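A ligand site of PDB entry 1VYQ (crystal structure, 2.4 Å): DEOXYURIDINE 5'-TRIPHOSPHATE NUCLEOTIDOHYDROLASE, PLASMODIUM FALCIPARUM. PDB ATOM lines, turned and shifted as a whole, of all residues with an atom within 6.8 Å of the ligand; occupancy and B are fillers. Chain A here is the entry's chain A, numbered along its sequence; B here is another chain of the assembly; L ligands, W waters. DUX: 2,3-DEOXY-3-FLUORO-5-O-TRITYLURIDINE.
An oxygen (O2) of the ligand sits at hydrogen-bond distance from the backbone NH of Ile 117 (3.1 Å). A nitrogen (N3) of the ligand lies within hydrogen-bond range of the backbone carbonyl oxygen (O) of Ile 117 (2.8 Å). An oxygen (O4) of the ligand is in hydrogen-bond range of the side-chain amide nitrogen of Asn 103.
The backbone NH (N) of Leu 88 lies within hydrogen-bond range of the backbone carbonyl oxygen (O) of Gly 106. O of Ser 92 of chain B is in hydrogen-bond range of OG of Ser 95 of chain B (2.7 Å). OG of Ser 93 of chain B is in hydrogen-bond range of NH1 of Arg 91 of chain B. The side-chain hydroxyl of Tyr 112 sits at hydrogen-bond distance from the backbone carbonyl oxygen of Glu 115, 2.6 Å away. The backbone carbonyl oxygen (O) of Ala 119 lies within hydrogen-bond range of the backbone NH (N) of Ala 102, at 2.8 Å.
Phe 46 touches the ligand (CD2 to C23, 3.5 Å). Leu 88 touches the ligand (CD2 to O4, 3.4 Å). CA of Gly 106 touches O4 of the ligand (3.2 Å). O of Leu 107 touches C6 of the ligand, at 3.9 Å. Tyr 112 touches the ligand. Ile 116 touches the ligand (CA to O2, 3.9 Å). Ala 119 touches the ligand (CB to C27, 3.9 Å). Ser 92 of chain B touches the ligand (OG to C6, 3.4 Å). Ser 93 of chain B touches the ligand. Ser 95 of chain B touches the ligand (OG to C26, 3.8 Å). Hydrophobic or aromatic side chains within 4 Å of the ligand: Phe 46, Leu 88, Tyr 112, Ile 117 and Ala 119. Within 4 Å of the ligand: Phe 46, Leu 88, Asn 103, Gly 106, Leu 107, Tyr 112, Ile 116, Ile 117, Ala 119, Ser 92 of chain B, Ser 93 of chain B and Ser 95 of chain B. The nearest printed residue that does not touch the ligand is Glu 115 (4.1 Å).
Water W1 lies within hydrogen-bond range of O4 of the ligand (2.7 Å), OD1 of Asn 103 (2.7 Å) and N of Ala 119 (3.0 Å).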
ATOM      1  N   PHE A  46      22.997 -12.550  -5.791  1.00  0.00           N
ATOM      2  CA  PHE A  46      23.481 -13.535  -4.854  1.00  0.00           C
ATOM      3  C   PHE A  46      24.851 -13.913  -5.337  1.00  0.00           C
ATOM      4  O   PHE A  46      25.015 -14.604  -6.353  1.00  0.00           O
ATOM      5  CB  PHE A  46      22.556 -14.717  -4.796  1.00  0.00           C
ATOM      6  CG  PHE A  46      21.193 -14.365  -4.345  1.00  0.00           C
ATOM      7  CD1 PHE A  46      20.217 -13.994  -5.265  1.00  0.00           C
ATOM      8  CD2 PHE A  46      20.895 -14.321  -2.995  1.00  0.00           C
ATOM      9  CE1 PHE A  46      18.964 -13.598  -4.841  1.00  0.00           C
ATOM     10  CE2 PHE A  46      19.648 -13.964  -2.563  1.00  0.00           C
ATOM     11  CZ  PHE A  46      18.657 -13.618  -3.491  1.00  0.00           C
ATOM     12  N   LYS A  48      28.146 -15.860  -4.956  1.00  0.00           N
ATOM     13  CA  LYS A  48      28.825 -17.040  -4.439  1.00  0.00           C
ATOM     14  C   LYS A  48      30.299 -16.804  -4.046  1.00  0.00           C
ATOM     15  O   LYS A  48      31.060 -16.292  -4.848  1.00  0.00           O
ATOM     16  CB  LYS A  48      28.762 -18.126  -5.544  1.00  0.00           C
ATOM     17  CG  LYS A  48      27.466 -18.914  -5.533  1.00  0.00           C
ATOM     18  CD  LYS A  48      27.168 -19.613  -6.831  1.00  0.00           C
ATOM     19  CE  LYS A  48      26.145 -20.726  -6.655  1.00  0.00           C
ATOM     20  NZ  LYS A  48      26.456 -21.931  -7.522  1.00  0.00           N
ATOM     21  N   LEU A  88      27.355 -13.864   9.133  1.00  0.00           N
ATOM     22  CA  LEU A  88      28.025 -13.271   7.981  1.00  0.00           C
ATOM     23  C   LEU A  88      27.717 -11.793   8.033  1.00  0.00           C
ATOM     24  O   LEU A  88      26.580 -11.364   7.802  1.00  0.00           O
ATOM     25  CB  LEU A  88      27.485 -13.925   6.688  1.00  0.00           C
ATOM     26  CG  LEU A  88      27.869 -13.385   5.297  1.00  0.00           C
ATOM     27  CD1 LEU A  88      29.284 -13.772   4.993  1.00  0.00           C
ATOM     28  CD2 LEU A  88      26.975 -13.989   4.235  1.00  0.00           C
ATOM     29  N   LEU A 101      24.098  -5.653   2.357  1.00  0.00           N
ATOM     30  CA  LEU A 101      23.658  -7.019   2.598  1.00  0.00           C
ATOM     31  C   LEU A 101      22.128  -7.009   2.710  1.00  0.00           C
ATOM     32  O   LEU A 101      21.570  -6.524   3.688  1.00  0.00           O
ATOM     33  CB  LEU A 101      24.279  -7.534   3.913  1.00  0.00           C
ATOM     34  CG  LEU A 101      25.365  -8.606   3.862  1.00  0.00           C
ATOM     35  CD1 LEU A 101      25.587  -9.220   5.218  1.00  0.00           C
ATOM     36  CD2 LEU A 101      25.016  -9.675   2.925  1.00  0.00           C
ATOM     37  N   ALA A 102      21.450  -7.529   1.692  1.00  0.00           N
ATOM     38  CA  ALA A 102      19.981  -7.567   1.665  1.00  0.00           C
ATOM     39  C   ALA A 102      19.337  -8.085   2.970  1.00  0.00           C
ATOM     40  O   ALA A 102      18.293  -7.555   3.427  1.00  0.00           O
ATOM     41  CB  ALA A 102      19.533  -8.437   0.513  1.00  0.00           C
ATOM     42  N   ASN A 103      19.954  -9.118   3.550  1.00  0.00           N
ATOM     43  CA  ASN A 103      19.418  -9.745   4.732  1.00  0.00           C
ATOM     44  C   ASN A 103      20.016  -9.203   6.037  1.00  0.00           C
ATOM     45  O   ASN A 103      19.797  -9.794   7.089  1.00  0.00           O
ATOM     46  CB  ASN A 103      19.474 -11.266   4.621  1.00  0.00           C
ATOM     47  CG  ASN A 103      20.851 -11.830   4.496  1.00  0.00           C
ATOM     48  OD1 ASN A 103      21.680 -11.344   3.711  1.00  0.00           O
ATOM     49  ND2 ASN A 103      21.083 -12.946   5.186  1.00  0.00           N
ATOM     50  N   ILE A 105      22.360  -9.107   8.288  1.00  0.00           N
ATOM     51  CA  ILE A 105      23.394  -9.998   8.723  1.00  0.00           C
ATOM     52  C   ILE A 105      22.940 -11.404   8.357  1.00  0.00           C
ATOM     53  O   ILE A 105      21.813 -11.770   8.635  1.00  0.00           O
ATOM     54  CB  ILE A 105      23.574  -9.897  10.226  1.00  0.00           C
ATOM     55  CG1 ILE A 105      23.810  -8.434  10.639  1.00  0.00           C
ATOM     56  CG2 ILE A 105      24.712 -10.836  10.698  1.00  0.00           C
ATOM     57  CD1 ILE A 105      25.174  -7.926  10.363  1.00  0.00           C
ATOM     58  N   GLY A 106      23.814 -12.124   7.649  1.00  0.00           N
ATOM     59  CA  GLY A 106      23.578 -13.504   7.342  1.00  0.00           C
ATOM     60  C   GLY A 106      23.651 -14.429   8.552  1.00  0.00           C
ATOM     61  O   GLY A 106      24.619 -14.399   9.312  1.00  0.00           O
ATOM     62  N   LEU A 107      22.626 -15.272   8.686  1.00  0.00           N
ATOM     63  CA  LEU A 107      22.573 -16.277   9.753  1.00  0.00           C
ATOM     64  C   LEU A 107      22.684 -17.655   9.167  1.00  0.00           C
ATOM     65  O   LEU A 107      21.804 -18.125   8.461  1.00  0.00           O
ATOM     66  CB  LEU A 107      21.290 -16.140  10.564  1.00  0.00           C
ATOM     67  CG  LEU A 107      21.032 -17.253  11.565  1.00  0.00           C
ATOM     68  CD1 LEU A 107      22.172 -17.452  12.485  1.00  0.00           C
ATOM     69  CD2 LEU A 107      19.782 -16.929  12.351  1.00  0.00           C
ATOM     70  N   ILE A 108      23.756 -18.319   9.467  1.00  0.00           N
ATOM     71  CA  ILE A 108      24.039 -19.553   8.791  1.00  0.00           C
ATOM     72  C   ILE A 108      23.811 -20.617   9.808  1.00  0.00           C
ATOM     73  O   ILE A 108      24.503 -20.641  10.786  1.00  0.00           O
ATOM     74  CB  ILE A 108      25.512 -19.517   8.283  1.00  0.00           C
ATOM     75  CG1 ILE A 108      25.675 -18.280   7.407  1.00  0.00           C
ATOM     76  CG2 ILE A 108      25.897 -20.843   7.576  1.00  0.00           C
ATOM     77  CD1 ILE A 108      27.008 -18.115   6.728  1.00  0.00           C
ATOM     78  N   ASP A 109      22.836 -21.498   9.606  1.00  0.00           N
ATOM     79  CA  ASP A 109      22.540 -22.499  10.631  1.00  0.00           C
ATOM     80  C   ASP A 109      23.650 -23.553  10.703  1.00  0.00           C
ATOM     81  O   ASP A 109      24.407 -23.783   9.752  1.00  0.00           O
ATOM     82  CB  ASP A 109      21.164 -23.173  10.451  1.00  0.00           C
ATOM     83  CG  ASP A 109      19.946 -22.191  10.626  1.00  0.00           C
ATOM     84  OD1 ASP A 109      19.742 -21.610  11.744  1.00  0.00           O
ATOM     85  OD2 ASP A 109      19.101 -21.965   9.699  1.00  0.00           O
ATOM     86  N   TYR A 112      23.890 -26.189   7.889  1.00  0.00           N
ATOM     87  CA  TYR A 112      24.228 -25.806   6.523  1.00  0.00           C
ATOM     88  C   TYR A 112      25.624 -26.267   6.121  1.00  0.00           C
ATOM     89  O   TYR A 112      26.605 -26.100   6.834  1.00  0.00           O
ATOM     90  CB  TYR A 112      24.042 -24.286   6.270  1.00  0.00           C
ATOM     91  CG  TYR A 112      24.137 -23.852   4.788  1.00  0.00           C
ATOM     92  CD1 TYR A 112      23.134 -24.179   3.862  1.00  0.00           C
ATOM     93  CD2 TYR A 112      25.221 -23.123   4.346  1.00  0.00           C
ATOM     94  CE1 TYR A 112      23.246 -23.813   2.544  1.00  0.00           C
ATOM     95  CE2 TYR A 112      25.350 -22.742   3.039  1.00  0.00           C
ATOM     96  CZ  TYR A 112      24.379 -23.061   2.127  1.00  0.00           C
ATOM     97  OH  TYR A 112      24.553 -22.651   0.822  1.00  0.00           O
ATOM     98  N   GLY A 114      26.256 -26.052   2.366  1.00  0.00           N
ATOM     99  CA  GLY A 114      26.386 -25.464   1.057  1.00  0.00           C
ATOM    100  C   GLY A 114      27.399 -24.319   0.948  1.00  0.00           C
ATOM    101  O   GLY A 114      27.972 -23.860   1.960  1.00  0.00           O
ATOM    102  N   GLU A 115      27.603 -23.890  -0.285  1.00  0.00           N
ATOM    103  CA  GLU A 115      28.408 -22.747  -0.596  1.00  0.00           C
ATOM    104  C   GLU A 115      27.858 -21.546   0.134  1.00  0.00           C
ATOM    105  O   GLU A 115      26.653 -21.336   0.206  1.00  0.00           O
ATOM    106  CB  GLU A 115      28.447 -22.462  -2.108  1.00  0.00           C
ATOM    107  CG  GLU A 115      29.500 -21.440  -2.559  1.00  0.00           C
ATOM    108  CD  GLU A 115      29.691 -21.438  -4.111  1.00  0.00           C
ATOM    109  OE1 GLU A 115      30.499 -20.609  -4.604  1.00  0.00           O
ATOM    110  OE2 GLU A 115      29.043 -22.241  -4.863  1.00  0.00           O
ATOM    111  N   ILE A 116      28.782 -20.740   0.623  1.00  0.00           N
ATOM    112  CA  ILE A 116      28.439 -19.510   1.276  1.00  0.00           C
ATOM    113  C   ILE A 116      28.226 -18.455   0.214  1.00  0.00           C
ATOM    114  O   ILE A 116      29.004 -18.353  -0.692  1.00  0.00           O
ATOM    115  CB  ILE A 116      29.514 -19.192   2.306  1.00  0.00           C
ATOM    116  CG1 ILE A 116      29.394 -20.192   3.457  1.00  0.00           C
ATOM    117  CG2 ILE A 116      29.325 -17.899   2.890  1.00  0.00           C
ATOM    118  CD1 ILE A 116      30.691 -20.327   4.152  1.00  0.00           C
ATOM    119  N   ILE A 117      27.199 -17.624   0.407  1.00  0.00           N
ATOM    120  CA  ILE A 117      26.671 -16.696  -0.571  1.00  0.00           C
ATOM    121  C   ILE A 117      26.323 -15.405   0.138  1.00  0.00           C
ATOM    122  O   ILE A 117      25.770 -15.397   1.203  1.00  0.00           O
ATOM    123  CB  ILE A 117      25.353 -17.291  -1.184  1.00  0.00           C
ATOM    124  CG1 ILE A 117      25.644 -18.492  -2.064  1.00  0.00           C
ATOM    125  CG2 ILE A 117      24.575 -16.277  -1.987  1.00  0.00           C
ATOM    126  CD1 ILE A 117      24.352 -19.180  -2.439  1.00  0.00           C
ATOM    127  N   ALA A 118      26.622 -14.289  -0.472  1.00  0.00           N
ATOM    128  CA  ALA A 118      26.213 -13.014   0.050  1.00  0.00           C
ATOM    129  C   ALA A 118      25.140 -12.409  -0.859  1.00  0.00           C
ATOM    130  O   ALA A 118      25.319 -12.351  -2.066  1.00  0.00           O
ATOM    131  CB  ALA A 118      27.437 -12.092   0.147  1.00  0.00           C
ATOM    132  N   ALA A 119      24.022 -11.970  -0.276  1.00  0.00           N
ATOM    133  CA  ALA A 119      22.988 -11.291  -1.051  1.00  0.00           C
ATOM    134  C   ALA A 119      23.238  -9.815  -1.052  1.00  0.00           C
ATOM    135  O   ALA A 119      22.773  -9.118  -0.176  1.00  0.00           O
ATOM    136  CB  ALA A 119      21.600 -11.554  -0.455  1.00  0.00           C
ATOM    137  N   ARG B  91      14.889 -12.800   7.739  1.00  0.00           N
ATOM    138  CA  ARG B  91      15.157 -14.123   7.250  1.00  0.00           C
ATOM    139  C   ARG B  91      15.931 -14.012   5.978  1.00  0.00           C
ATOM    140  O   ARG B  91      15.878 -12.982   5.330  1.00  0.00           O
ATOM    141  CB  ARG B  91      13.867 -14.859   6.994  1.00  0.00           C
ATOM    142  CG  ARG B  91      13.280 -15.405   8.215  1.00  0.00           C
ATOM    143  CD  ARG B  91      11.983 -15.967   7.960  1.00  0.00           C
ATOM    144  NE  ARG B  91      12.077 -17.403   7.721  1.00  0.00           N
ATOM    145  CZ  ARG B  91      11.638 -18.028   6.646  1.00  0.00           C
ATOM    146  NH1 ARG B  91      11.143 -17.387   5.602  1.00  0.00           N
ATOM    147  NH2 ARG B  91      11.777 -19.348   6.596  1.00  0.00           N
ATOM    148  N   SER B  92      16.691 -15.055   5.664  1.00  0.00           N
ATOM    149  CA  SER B  92      17.432 -15.129   4.417  1.00  0.00           C
ATOM    150  C   SER B  92      16.520 -14.788   3.245  1.00  0.00           C
ATOM    151  O   SER B  92      16.942 -14.131   2.309  1.00  0.00           O
ATOM    152  CB  SER B  92      17.998 -16.522   4.219  1.00  0.00           C
ATOM    153  OG  SER B  92      19.081 -16.749   5.096  1.00  0.00           O
ATOM    154  N   SER B  93      15.264 -15.219   3.355  1.00  0.00           N
ATOM    155  CA  SER B  93      14.284 -15.142   2.262  1.00  0.00           C
ATOM    156  C   SER B  93      13.788 -13.755   1.960  1.00  0.00           C
ATOM    157  O   SER B  93      13.251 -13.508   0.889  1.00  0.00           O
ATOM    158  CB  SER B  93      13.084 -16.058   2.587  1.00  0.00           C
ATOM    159  OG  SER B  93      12.368 -15.601   3.709  1.00  0.00           O
ATOM    160  N   ILE B  94      13.932 -12.851   2.907  1.00  0.00           N
ATOM    161  CA  ILE B  94      13.557 -11.451   2.676  1.00  0.00           C
ATOM    162  C   ILE B  94      14.252 -10.831   1.431  1.00  0.00           C
ATOM    163  O   ILE B  94      13.791  -9.850   0.873  1.00  0.00           O
ATOM    164  CB  ILE B  94      13.863 -10.599   3.961  1.00  0.00           C
ATOM    165  CG1 ILE B  94      12.885  -9.424   4.028  1.00  0.00           C
ATOM    166  CG2 ILE B  94      15.351 -10.147   3.975  1.00  0.00           C
ATOM    167  CD1 ILE B  94      12.975  -8.595   5.216  1.00  0.00           C
ATOM    168  N   SER B  95      15.369 -11.419   1.033  1.00  0.00           N
ATOM    169  CA  SER B  95      16.203 -10.868   0.002  1.00  0.00           C
ATOM    170  C   SER B  95      15.673 -11.103  -1.419  1.00  0.00           C
ATOM    171  O   SER B  95      16.136 -10.451  -2.365  1.00  0.00           O
ATOM    172  CB  SER B  95      17.596 -11.449   0.144  1.00  0.00           C
ATOM    173  OG  SER B  95      17.462 -12.832  -0.006  1.00  0.00           O
ATOM    174  N   LYS B  96      14.732 -12.029  -1.568  1.00  0.00           N
ATOM    175  CA  LYS B  96      13.884 -12.171  -2.730  1.00  0.00           C
ATOM    176  C   LYS B  96      12.681 -11.233  -2.633  1.00  0.00           C
ATOM    177  O   LYS B  96      11.588 -11.534  -3.092  1.00  0.00           O
ATOM    178  CB  LYS B  96      13.410 -13.617  -2.813  1.00  0.00           C
ATOM    179  CG  LYS B  96      14.040 -14.378  -3.988  1.00  0.00           C
HETATM  180  F3' DUX L   1      20.203 -21.650   4.243  1.00  0.00           F
HETATM  181  C3' DUX L   1      20.838 -20.484   4.080  1.00  0.00           C
HETATM  182  C2' DUX L   1      22.240 -20.548   4.683  1.00  0.00           C
HETATM  183  C1' DUX L   1      23.053 -19.794   3.652  1.00  0.00           C
HETATM  184  N1  DUX L   1      23.151 -18.353   3.865  1.00  0.00           N
HETATM  185  C2  DUX L   1      24.182 -17.648   3.187  1.00  0.00           C
HETATM  186  N3  DUX L   1      24.327 -16.318   3.371  1.00  0.00           N
HETATM  187  C4  DUX L   1      23.470 -15.617   4.170  1.00  0.00           C
HETATM  188  C5  DUX L   1      22.429 -16.255   4.834  1.00  0.00           C
HETATM  189  C6  DUX L   1      22.298 -17.640   4.670  1.00  0.00           C
HETATM  190  O4  DUX L   1      23.576 -14.387   4.297  1.00  0.00           O
HETATM  191  O2  DUX L   1      24.962 -18.298   2.441  1.00  0.00           O
HETATM  192  O4' DUX L   1      22.376 -19.967   2.403  1.00  0.00           O
HETATM  193  C4' DUX L   1      20.966 -20.272   2.597  1.00  0.00           C
HETATM  194  C5' DUX L   1      19.990 -19.220   2.095  1.00  0.00           C
HETATM  195  O5' DUX L   1      19.740 -19.390   0.664  1.00  0.00           O
HETATM  196  C17 DUX L   1      19.323 -18.259  -0.163  1.00  0.00           C
HETATM  197  C30 DUX L   1      17.808 -18.130  -0.035  1.00  0.00           C
HETATM  198  C31 DUX L   1      17.050 -18.971   0.824  1.00  0.00           C
HETATM  199  C32 DUX L   1      15.663 -18.839   0.914  1.00  0.00           C
HETATM  200  C33 DUX L   1      14.988 -17.899   0.122  1.00  0.00           C
HETATM  201  C34 DUX L   1      15.705 -17.098  -0.750  1.00  0.00           C
HETATM  202  C35 DUX L   1      17.110 -17.193  -0.826  1.00  0.00           C
HETATM  203  C24 DUX L   1      20.124 -17.078   0.345  1.00  0.00           C
HETATM  204  C25 DUX L   1      19.539 -15.953   0.928  1.00  0.00           C
HETATM  205  C26 DUX L   1      20.313 -14.903   1.418  1.00  0.00           C
HETATM  206  C27 DUX L   1      21.698 -14.975   1.370  1.00  0.00           C
HETATM  207  C28 DUX L   1      22.314 -16.082   0.801  1.00  0.00           C
HETATM  208  C29 DUX L   1      21.544 -17.134   0.297  1.00  0.00           C
HETATM  209  C18 DUX L   1      19.661 -18.615  -1.611  1.00  0.00           C
HETATM  210  C19 DUX L   1      19.476 -19.927  -2.084  1.00  0.00           C
HETATM  211  C20 DUX L   1      19.781 -20.257  -3.427  1.00  0.00           C
HETATM  212  C21 DUX L   1      20.296 -19.296  -4.315  1.00  0.00           C
HETATM  213  C22 DUX L   1      20.464 -17.989  -3.853  1.00  0.00           C
HETATM  214  C23 DUX L   1      20.164 -17.671  -2.523  1.00  0.00           C
HETATM  215  O   HOH W   1      24.032 -12.296   2.701  1.00  0.00           O
HETATM  216  O   HOH W   2      18.844 -22.569   0.103  1.00  0.00           O
